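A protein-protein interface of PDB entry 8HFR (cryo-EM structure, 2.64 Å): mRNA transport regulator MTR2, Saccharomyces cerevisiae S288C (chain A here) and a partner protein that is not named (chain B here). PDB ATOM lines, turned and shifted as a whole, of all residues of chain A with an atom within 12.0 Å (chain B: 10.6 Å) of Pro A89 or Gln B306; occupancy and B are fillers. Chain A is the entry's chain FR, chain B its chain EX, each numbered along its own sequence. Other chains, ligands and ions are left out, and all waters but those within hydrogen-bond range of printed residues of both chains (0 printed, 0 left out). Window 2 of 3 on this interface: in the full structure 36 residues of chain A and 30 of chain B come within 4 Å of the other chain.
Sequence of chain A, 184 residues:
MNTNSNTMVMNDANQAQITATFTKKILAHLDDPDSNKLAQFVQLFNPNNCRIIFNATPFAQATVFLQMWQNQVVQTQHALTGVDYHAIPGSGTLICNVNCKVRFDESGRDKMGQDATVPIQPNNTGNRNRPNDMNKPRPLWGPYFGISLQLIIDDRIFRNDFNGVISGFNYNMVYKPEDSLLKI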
ATOM      1  N   MET A   8     -20.869  20.537  16.468  1.00  0.00           N
ATOM      2  CA  MET A   8     -21.023  21.088  17.809  1.00  0.00           C
ATOM      3  C   MET A   8     -20.314  22.431  17.928  1.00  0.00           C
ATOM      4  O   MET A   8     -20.095  23.119  16.933  1.00  0.00           O
ATOM      5  CB  MET A   8     -20.491  20.112  18.845  1.00  0.00           C
ATOM      6  N   VAL A   9     -19.971  22.803  19.156  1.00  0.00           N
ATOM      7  CA  VAL A   9     -19.169  23.981  19.434  1.00  0.00           C
ATOM      8  C   VAL A   9     -17.736  23.544  19.740  1.00  0.00           C
ATOM      9  O   VAL A   9     -17.383  22.366  19.609  1.00  0.00           O
ATOM     10  CB  VAL A   9     -19.787  24.785  20.577  1.00  0.00           C
ATOM     11  N   MET A  10     -16.899  24.494  20.151  1.00  0.00           N
ATOM     12  CA  MET A  10     -15.491  24.199  20.380  1.00  0.00           C
ATOM     13  C   MET A  10     -14.915  25.186  21.383  1.00  0.00           C
ATOM     14  O   MET A  10     -15.551  26.171  21.765  1.00  0.00           O
ATOM     15  CB  MET A  10     -14.689  24.239  19.074  1.00  0.00           C
ATOM     16  N   ASN A  11     -13.690  24.886  21.815  1.00  0.00           N
ATOM     17  CA  ASN A  11     -12.870  25.785  22.626  1.00  0.00           C
ATOM     18  C   ASN A  11     -11.415  25.464  22.277  1.00  0.00           C
ATOM     19  O   ASN A  11     -10.809  24.572  22.873  1.00  0.00           O
ATOM     20  CB  ASN A  11     -13.150  25.607  24.110  1.00  0.00           C
ATOM     21  N   TYR A  85     -12.856  34.337  15.058  1.00  0.00           N
ATOM     22  CA  TYR A  85     -13.481  33.250  14.317  1.00  0.00           C
ATOM     23  C   TYR A  85     -14.761  32.794  15.008  1.00  0.00           C
ATOM     24  O   TYR A  85     -15.021  33.119  16.168  1.00  0.00           O
ATOM     25  CB  TYR A  85     -12.523  32.060  14.155  1.00  0.00           C
ATOM     26  N   HIS A  86     -15.563  32.033  14.264  1.00  0.00           N
ATOM     27  CA  HIS A  86     -16.812  31.468  14.750  1.00  0.00           C
ATOM     28  C   HIS A  86     -17.018  30.099  14.116  1.00  0.00           C
ATOM     29  O   HIS A  86     -16.854  29.940  12.901  1.00  0.00           O
ATOM     30  CB  HIS A  86     -17.991  32.395  14.424  1.00  0.00           C
ATOM     31  N   ALA A  87     -17.381  29.115  14.942  1.00  0.00           N
ATOM     32  CA  ALA A  87     -17.468  27.717  14.533  1.00  0.00           C
ATOM     33  C   ALA A  87     -18.880  27.189  14.752  1.00  0.00           C
ATOM     34  O   ALA A  87     -19.362  27.152  15.888  1.00  0.00           O
ATOM     35  CB  ALA A  87     -16.466  26.860  15.304  1.00  0.00           C
ATOM     36  N   ILE A  88     -19.518  26.738  13.672  1.00  0.00           N
ATOM     37  CA  ILE A  88     -20.911  26.327  13.687  1.00  0.00           C
ATOM     38  C   ILE A  88     -21.036  24.818  13.890  1.00  0.00           C
ATOM     39  O   ILE A  88     -20.055  24.114  14.150  1.00  0.00           O
ATOM     40  CB  ILE A  88     -21.593  26.772  12.392  1.00  0.00           C
ATOM     41  N   PRO A  89     -22.268  24.313  13.778  1.00  0.00           N
ATOM     42  CA  PRO A  89     -22.572  22.893  13.864  1.00  0.00           C
ATOM     43  C   PRO A  89     -23.422  22.491  12.668  1.00  0.00           C
ATOM     44  O   PRO A  89     -24.034  23.337  12.007  1.00  0.00           O
ATOM     45  CB  PRO A  89     -23.309  22.542  15.161  1.00  0.00           C
ATOM     46  N   GLY A  90     -23.406  21.183  12.378  1.00  0.00           N
ATOM     47  CA  GLY A  90     -24.094  20.453  11.302  1.00  0.00           C
ATOM     48  C   GLY A  90     -23.572  20.789   9.907  1.00  0.00           C
ATOM     49  O   GLY A  90     -24.027  20.180   8.930  1.00  0.00           O
ATOM     50  N   SER A  91     -22.643  21.734   9.782  1.00  0.00           N
ATOM     51  CA  SER A  91     -21.901  21.976   8.553  1.00  0.00           C
ATOM     52  C   SER A  91     -20.427  22.228   8.802  1.00  0.00           C
ATOM     53  O   SER A  91     -19.666  22.271   7.829  1.00  0.00           O
ATOM     54  CB  SER A  91     -22.495  23.166   7.786  1.00  0.00           C
ATOM     55  N   GLY A  92     -20.006  22.386  10.068  1.00  0.00           N
ATOM     56  CA  GLY A  92     -18.636  22.722  10.483  1.00  0.00           C
ATOM     57  C   GLY A  92     -18.128  23.992   9.804  1.00  0.00           C
ATOM     58  O   GLY A  92     -16.953  24.092   9.441  1.00  0.00           O
ATOM     59  N   THR A  93     -19.016  24.967   9.630  1.00  0.00           N
ATOM     60  CA  THR A  93     -18.676  26.199   8.937  1.00  0.00           C
ATOM     61  C   THR A  93     -17.822  27.082   9.837  1.00  0.00           C
ATOM     62  O   THR A  93     -18.178  27.337  10.992  1.00  0.00           O
ATOM     63  CB  THR A  93     -19.947  26.929   8.505  1.00  0.00           C
ATOM     64  N   LEU A  94     -16.685  27.534   9.310  1.00  0.00           N
ATOM     65  CA  LEU A  94     -15.727  28.345  10.055  1.00  0.00           C
ATOM     66  C   LEU A  94     -15.706  29.740   9.444  1.00  0.00           C
ATOM     67  O   LEU A  94     -15.128  29.947   8.375  1.00  0.00           O
ATOM     68  CB  LEU A  94     -14.339  27.712  10.032  1.00  0.00           C
ATOM     69  N   ILE A  95     -16.357  30.687  10.112  1.00  0.00           N
ATOM     70  CA  ILE A  95     -16.462  32.057   9.628  1.00  0.00           C
ATOM     71  C   ILE A  95     -15.550  32.925  10.481  1.00  0.00           C
ATOM     72  O   ILE A  95     -15.830  33.157  11.658  1.00  0.00           O
ATOM     73  CB  ILE A  95     -17.905  32.555   9.683  1.00  0.00           C
ATOM     74  N   ILE A 152     -15.742  32.907   5.279  1.00  0.00           N
ATOM     75  CA  ILE A 152     -16.398  31.689   5.729  1.00  0.00           C
ATOM     76  C   ILE A 152     -15.895  30.538   4.868  1.00  0.00           C
ATOM     77  O   ILE A 152     -16.046  30.559   3.636  1.00  0.00           O
ATOM     78  CB  ILE A 152     -17.921  31.814   5.658  1.00  0.00           C
ATOM     79  N   ILE A 153     -15.289  29.553   5.525  1.00  0.00           N
ATOM     80  CA  ILE A 153     -14.593  28.450   4.889  1.00  0.00           C
ATOM     81  C   ILE A 153     -14.867  27.190   5.701  1.00  0.00           C
ATOM     82  O   ILE A 153     -15.730  27.168   6.586  1.00  0.00           O
ATOM     83  CB  ILE A 153     -13.093  28.753   4.782  1.00  0.00           C
ATOM     84  N   ASP A 154     -14.112  26.136   5.411  1.00  0.00           N
ATOM     85  CA  ASP A 154     -14.318  24.846   6.047  1.00  0.00           C
ATOM     86  C   ASP A 154     -13.620  24.785   7.403  1.00  0.00           C
ATOM     87  O   ASP A 154     -12.842  25.667   7.780  1.00  0.00           O
ATOM     88  CB  ASP A 154     -13.813  23.722   5.142  1.00  0.00           C
ATOM     89  N   ASP A 155     -13.915  23.716   8.146  1.00  0.00           N
ATOM     90  CA  ASP A 155     -13.153  23.354   9.334  1.00  0.00           C
ATOM     91  C   ASP A 155     -11.906  22.546   9.000  1.00  0.00           C
ATOM     92  O   ASP A 155     -11.169  22.156   9.912  1.00  0.00           O
ATOM     93  CB  ASP A 155     -14.029  22.570  10.312  1.00  0.00           C
ATOM     94  N   LEU B 300     -32.915  34.531  22.009  1.00  0.00           N
ATOM     95  CA  LEU B 300     -32.971  33.104  22.312  1.00  0.00           C
ATOM     96  C   LEU B 300     -33.779  32.341  21.269  1.00  0.00           C
ATOM     97  O   LEU B 300     -33.556  31.143  21.064  1.00  0.00           O
ATOM     98  CB  LEU B 300     -33.550  32.889  23.711  1.00  0.00           C
ATOM     99  N   LEU B 302     -33.749  33.105  17.978  1.00  0.00           N
ATOM    100  CA  LEU B 302     -32.870  33.014  16.824  1.00  0.00           C
ATOM    101  C   LEU B 302     -31.440  32.636  17.198  1.00  0.00           C
ATOM    102  O   LEU B 302     -30.517  32.921  16.432  1.00  0.00           O
ATOM    103  CB  LEU B 302     -32.884  34.329  16.042  1.00  0.00           C
ATOM    104  N   TYR B 303     -31.235  32.021  18.360  1.00  0.00           N
ATOM    105  CA  TYR B 303     -29.951  31.420  18.710  1.00  0.00           C
ATOM    106  C   TYR B 303     -30.157  29.945  19.030  1.00  0.00           C
ATOM    107  O   TYR B 303     -31.024  29.594  19.836  1.00  0.00           O
ATOM    108  CB  TYR B 303     -29.303  32.138  19.899  1.00  0.00           C
ATOM    109  N   SER B 304     -29.364  29.088  18.392  1.00  0.00           N
ATOM    110  CA  SER B 304     -29.389  27.658  18.660  1.00  0.00           C
ATOM    111  C   SER B 304     -28.427  27.319  19.791  1.00  0.00           C
ATOM    112  O   SER B 304     -27.681  28.169  20.275  1.00  0.00           O
ATOM    113  CB  SER B 304     -29.034  26.868  17.403  1.00  0.00           C
ATOM    114  N   PRO B 305     -28.436  26.046  20.198  1.00  0.00           N
ATOM    115  CA  PRO B 305     -27.633  25.620  21.342  1.00  0.00           C
ATOM    116  C   PRO B 305     -26.141  25.656  21.030  1.00  0.00           C
ATOM    117  O   PRO B 305     -25.332  26.067  21.871  1.00  0.00           O
ATOM    118  CB  PRO B 305     -28.051  24.217  21.781  1.00  0.00           C
ATOM    119  N   GLN B 306     -25.759  25.254  19.820  1.00  0.00           N
ATOM    120  CA  GLN B 306     -24.361  25.195  19.400  1.00  0.00           C
ATOM    121  C   GLN B 306     -23.969  26.413  18.572  1.00  0.00           C
ATOM    122  O   GLN B 306     -23.247  26.291  17.576  1.00  0.00           O
ATOM    123  CB  GLN B 306     -24.089  23.905  18.633  1.00  0.00           C
ATOM    124  N   SER B 307     -24.458  27.592  18.962  1.00  0.00           N
ATOM    125  CA  SER B 307     -24.238  28.829  18.222  1.00  0.00           C
ATOM    126  C   SER B 307     -22.763  29.232  18.220  1.00  0.00           C
ATOM    127  O   SER B 307     -21.941  28.720  18.987  1.00  0.00           O
ATOM    128  CB  SER B 307     -25.081  29.958  18.812  1.00  0.00           C
ATOM    129  N   GLN B 308     -22.434  30.177  17.339  1.00  0.00           N
ATOM    130  CA  GLN B 308     -21.058  30.590  17.074  1.00  0.00           C
ATOM    131  C   GLN B 308     -20.940  32.101  17.254  1.00  0.00           C
ATOM    132  O   GLN B 308     -21.183  32.871  16.322  1.00  0.00           O
ATOM    133  CB  GLN B 308     -20.638  30.168  15.675  1.00  0.00           C
ATOM    134  N   PHE B 309     -20.566  32.520  18.457  1.00  0.00           N
ATOM    135  CA  PHE B 309     -20.331  33.921  18.764  1.00  0.00           C
ATOM    136  C   PHE B 309     -18.836  34.209  18.816  1.00  0.00           C
ATOM    137  O   PHE B 309     -18.001  33.302  18.849  1.00  0.00           O
ATOM    138  CB  PHE B 309     -20.996  34.303  20.090  1.00  0.00           C
ATOM    139  N   SER B 310     -18.509  35.498  18.823  1.00  0.00           N
ATOM    140  CA  SER B 310     -17.131  35.960  18.964  1.00  0.00           C
ATOM    141  C   SER B 310     -17.162  37.388  19.492  1.00  0.00           C
ATOM    142  O   SER B 310     -18.228  37.981  19.681  1.00  0.00           O
ATOM    143  CB  SER B 310     -16.364  35.871  17.640  1.00  0.00           C
ATOM    144  N   SER B 355     -16.633  31.695  22.746  1.00  0.00           N
ATOM    145  CA  SER B 355     -17.984  32.241  22.755  1.00  0.00           C
ATOM    146  C   SER B 355     -18.924  31.318  21.983  1.00  0.00           C
ATOM    147  O   SER B 355     -18.898  31.275  20.749  1.00  0.00           O
ATOM    148  CB  SER B 355     -17.981  33.656  22.183  1.00  0.00           C
ATOM    149  N   ILE B 356     -19.745  30.582  22.722  1.00  0.00           N
ATOM    150  CA  ILE B 356     -20.789  29.706  22.202  1.00  0.00           C
ATOM    151  C   ILE B 356     -21.896  29.667  23.250  1.00  0.00           C
ATOM    152  O   ILE B 356     -21.986  30.571  24.089  1.00  0.00           O
ATOM    153  CB  ILE B 356     -20.216  28.319  21.866  1.00  0.00           C
ATOM    154  N   GLY B 357     -22.750  28.636  23.182  1.00  0.00           N
ATOM    155  CA  GLY B 357     -23.648  28.227  24.271  1.00  0.00           C
ATOM    156  C   GLY B 357     -24.658  29.327  24.626  1.00  0.00           C
ATOM    157  O   GLY B 357     -24.515  30.029  25.624  1.00  0.00           O
ATOM    158  N   GLN B 358     -25.658  29.469  23.741  1.00  0.00           N
ATOM    159  CA  GLN B 358     -26.615  30.580  23.631  1.00  0.00           C
ATOM    160  C   GLN B 358     -27.138  31.200  24.923  1.00  0.00           C
ATOM    161  O   GLN B 358     -27.343  32.414  24.972  1.00  0.00           O
ATOM    162  CB  GLN B 358     -27.830  30.132  22.823  1.00  0.00           C
ATOM    163  N   GLU B 359     -27.335  30.399  25.973  1.00  0.00           N
ATOM    164  CA  GLU B 359     -27.615  30.963  27.292  1.00  0.00           C
ATOM    165  C   GLU B 359     -26.418  31.755  27.811  1.00  0.00           C
ATOM    166  O   GLU B 359     -26.548  32.925  28.198  1.00  0.00           O
ATOM    167  CB  GLU B 359     -27.996  29.850  28.268  1.00  0.00           C
ATOM    168  N   SER B 360     -25.225  31.149  27.775  1.00  0.00           N
ATOM    169  CA  SER B 360     -24.014  31.869  28.154  1.00  0.00           C
ATOM    170  C   SER B 360     -23.628  32.930  27.130  1.00  0.00           C
ATOM    171  O   SER B 360     -22.911  33.866  27.474  1.00  0.00           O
ATOM    172  CB  SER B 360     -22.853  30.893  28.362  1.00  0.00           C
ATOM    173  N   ILE B 361     -24.131  32.838  25.899  1.00  0.00           N
ATOM    174  CA  ILE B 361     -23.839  33.857  24.895  1.00  0.00           C
ATOM    175  C   ILE B 361     -24.742  35.077  25.064  1.00  0.00           C
ATOM    176  O   ILE B 361     -24.312  36.211  24.826  1.00  0.00           O
ATOM    177  CB  ILE B 361     -23.978  33.269  23.494  1.00  0.00           C
ATOM    178  N   GLN B 391     -23.257  25.970   1.469  1.00  0.00           N
ATOM    179  CA  GLN B 391     -22.721  24.824   2.191  1.00  0.00           C
ATOM    180  C   GLN B 391     -23.672  24.400   3.299  1.00  0.00           C
ATOM    181  O   GLN B 391     -23.943  23.208   3.479  1.00  0.00           O
ATOM    182  CB  GLN B 391     -21.340  25.149   2.761  1.00  0.00           C
ATOM    183  N   ILE B 392     -24.193  25.373   4.044  1.00  0.00           N
ATOM    184  CA  ILE B 392     -25.166  25.141   5.100  1.00  0.00           C
ATOM    185  C   ILE B 392     -26.574  25.549   4.688  1.00  0.00           C
ATOM    186  O   ILE B 392     -27.487  25.486   5.519  1.00  0.00           O
ATOM    187  CB  ILE B 392     -24.753  25.887   6.371  1.00  0.00           C
ATOM    188  N   ASN B 393     -26.753  25.949   3.419  1.00  0.00           N
ATOM    189  CA  ASN B 393     -28.014  26.455   2.852  1.00  0.00           C
ATOM    190  C   ASN B 393     -28.552  27.642   3.652  1.00  0.00           C
ATOM    191  O   ASN B 393     -29.727  27.694   4.020  1.00  0.00           O
ATOM    192  CB  ASN B 393     -29.065  25.344   2.722  1.00  0.00           C
ATOM    193  N   GLY B 394     -27.677  28.616   3.907  1.00  0.00           N
ATOM    194  CA  GLY B 394     -28.004  29.748   4.765  1.00  0.00           C
ATOM    195  C   GLY B 394     -27.603  31.048   4.075  1.00  0.00           C
ATOM    196  O   GLY B 394     -27.178  31.060   2.917  1.00  0.00           O
ATOM    197  N   VAL B 450     -25.068  34.846  10.268  1.00  0.00           N
ATOM    198  CA  VAL B 450     -25.431  33.752   9.379  1.00  0.00           C
ATOM    199  C   VAL B 450     -26.682  33.074   9.918  1.00  0.00           C
ATOM    200  O   VAL B 450     -26.687  32.577  11.049  1.00  0.00           O
ATOM    201  CB  VAL B 450     -24.292  32.738   9.244  1.00  0.00           C
ATOM    202  N   VAL B 452     -30.236  30.599   8.566  1.00  0.00           N
ATOM    203  CA  VAL B 452     -30.825  29.763   7.531  1.00  0.00           C
ATOM    204  C   VAL B 452     -32.210  30.283   7.176  1.00  0.00           C
ATOM    205  O   VAL B 452     -32.750  31.157   7.863  1.00  0.00           O
ATOM    206  CB  VAL B 452     -30.902  28.308   7.991  1.00  0.00           C
ATOM    207  N   ILE B 459     -33.041  30.267  12.352  1.00  0.00           N
ATOM    208  CA  ILE B 459     -31.967  29.453  12.909  1.00  0.00           C
ATOM    209  C   ILE B 459     -30.641  30.080  12.495  1.00  0.00           C
ATOM    210  O   ILE B 459     -30.199  29.920  11.357  1.00  0.00           O
ATOM    211  CB  ILE B 459     -32.075  28.006  12.440  1.00  0.00           C
ATOM    212  N   ILE B 460     -30.017  30.801  13.418  1.00  0.00           N
ATOM    213  CA  ILE B 460     -28.724  31.419  13.173  1.00  0.00           C
ATOM    214  C   ILE B 460     -27.623  30.594  13.817  1.00  0.00           C
ATOM    215  O   ILE B 460     -27.814  29.983  14.870  1.00  0.00           O
ATOM    216  CB  ILE B 460     -28.680  32.850  13.711  1.00  0.00           C
ATOM    217  N   ALA B 461     -26.463  30.576  13.164  1.00  0.00           N
ATOM    218  CA  ALA B 461     -25.291  29.905  13.709  1.00  0.00           C
ATOM    219  C   ALA B 461     -24.173  30.886  14.037  1.00  0.00           C
ATOM    220  O   ALA B 461     -23.781  31.007  15.201  1.00  0.00           O
ATOM    221  CB  ALA B 461     -24.787  28.833  12.731  1.00  0.00           C
ATOM    222  N   SER B 462     -23.690  31.632  13.048  1.00  0.00           N
ATOM    223  CA  SER B 462     -22.511  32.481  13.190  1.00  0.00           C
ATOM    224  C   SER B 462     -22.965  33.920  13.401  1.00  0.00           C
ATOM    225  O   SER B 462     -23.220  34.646  12.440  1.00  0.00           O
ATOM    226  CB  SER B 462     -21.606  32.355  11.969  1.00  0.00           C
ATOM    227  N   ASP B 463     -23.069  34.328  14.664  1.00  0.00           N
ATOM    228  CA  ASP B 463     -23.459  35.689  15.031  1.00  0.00           C
ATOM    229  C   ASP B 463     -22.364  36.244  15.936  1.00  0.00           C
ATOM    230  O   ASP B 463     -22.341  35.963  17.138  1.00  0.00           O
ATOM    231  CB  ASP B 463     -24.820  35.714  15.715  1.00  0.00           C
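The backbone NH of His A86 sits at hydrogen-bond distance from the backbone carbonyl oxygen of Ile A95.
The backbone NH (N) of Ile A88 is in hydrogen-bond range of the backbone carbonyl oxygen (O) of Thr A93.
The backbone carbonyl oxygen of Ala B461 sits at hydrogen-bond distance from the backbone NH of Gln B308 (2.7 Å).
N of Asp B463 is in hydrogen-bond range of O of Gln B308, at 2.9 Å.
The backbone carbonyl oxygen (O) of Val B450 is in hydrogen-bond range of the backbone NH (N) of Ala B461.
Val A9 touches Ile B356 (CB to CB, 3.8 Å).
O of Tyr A85 touches CB of Ser B310, at 3.4 Å.
CB of Gln B308 touches CB of His A86, at 3.7 Å.
O of Ala A87 touches CB of Gln B308 (3.3 Å).
Ile A88 touches Ala B461.
Pro A89 touches Gln B306 (CB to CB, 3.8 Å).
CB of Ser A91 touches CB of Ile B392, 3.8 Å away.
Met A8 touches none of the printed residues of chain B.
Printed residues of chain B within 4 Å of Val A9: Ile B356.
Printed residues of chain B within 4 Å of His A86: Gln B308 (3.7 Å).
Of the printed residues of chain B, Ala A87 touches Gln B308 (3.3 Å).
Ile A88 touches just one residue of chain B: Ala B461.
Pro A89 touches just one residue of chain B: Gln B306.
No residue of chain B comes within 4 Å of Gly A90.
Of chain B, only Ile B392 comes within 4 Å of Ser A91.
No residue of chain A comes within 4 Å of Ser B304.
Of the printed residues of chain A, Gln B306 touches Pro A89 (3.8 Å).
Ser B307 touches none of the printed residues of chain A.
Of chain A, only His A86 (3.7 Å) and Ala A87 (3.3 Å) come within 4 Å of Gln B308.
Printed residues of chain A within 4 Å of Ser B310: Tyr A85 (3.4 Å).
Of chain A, only Val A9 (3.8 Å) comes within 4 Å of Ile B356.
No residue of chain A comes within 4 Å of Gly B357.
Gln B358 touches none of the printed residues of chain A.
Of the printed residues of chain A, Ile B392 touches Ser A91 (3.8 Å).
Of chain A, only Ile A88 (3.8 Å) comes within 4 Å of Ala B461.
Ser B462 touches none of the printed residues of chain A.
The nearest residue of chain A that does not touch Gln B306 is Met A8 (4.1 Å).
Hydrophobic or aromatic side chains of chain A that line the printed part of chain B: Val A9, His A86, Ile A88 and Pro A89.
Among the printed residues, 7 pairs touch across the chains.
Among the printed residues, no Asp or Glu carboxylate lies within 4 Å of a Lys or Arg side-chain nitrogen of the other chain.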
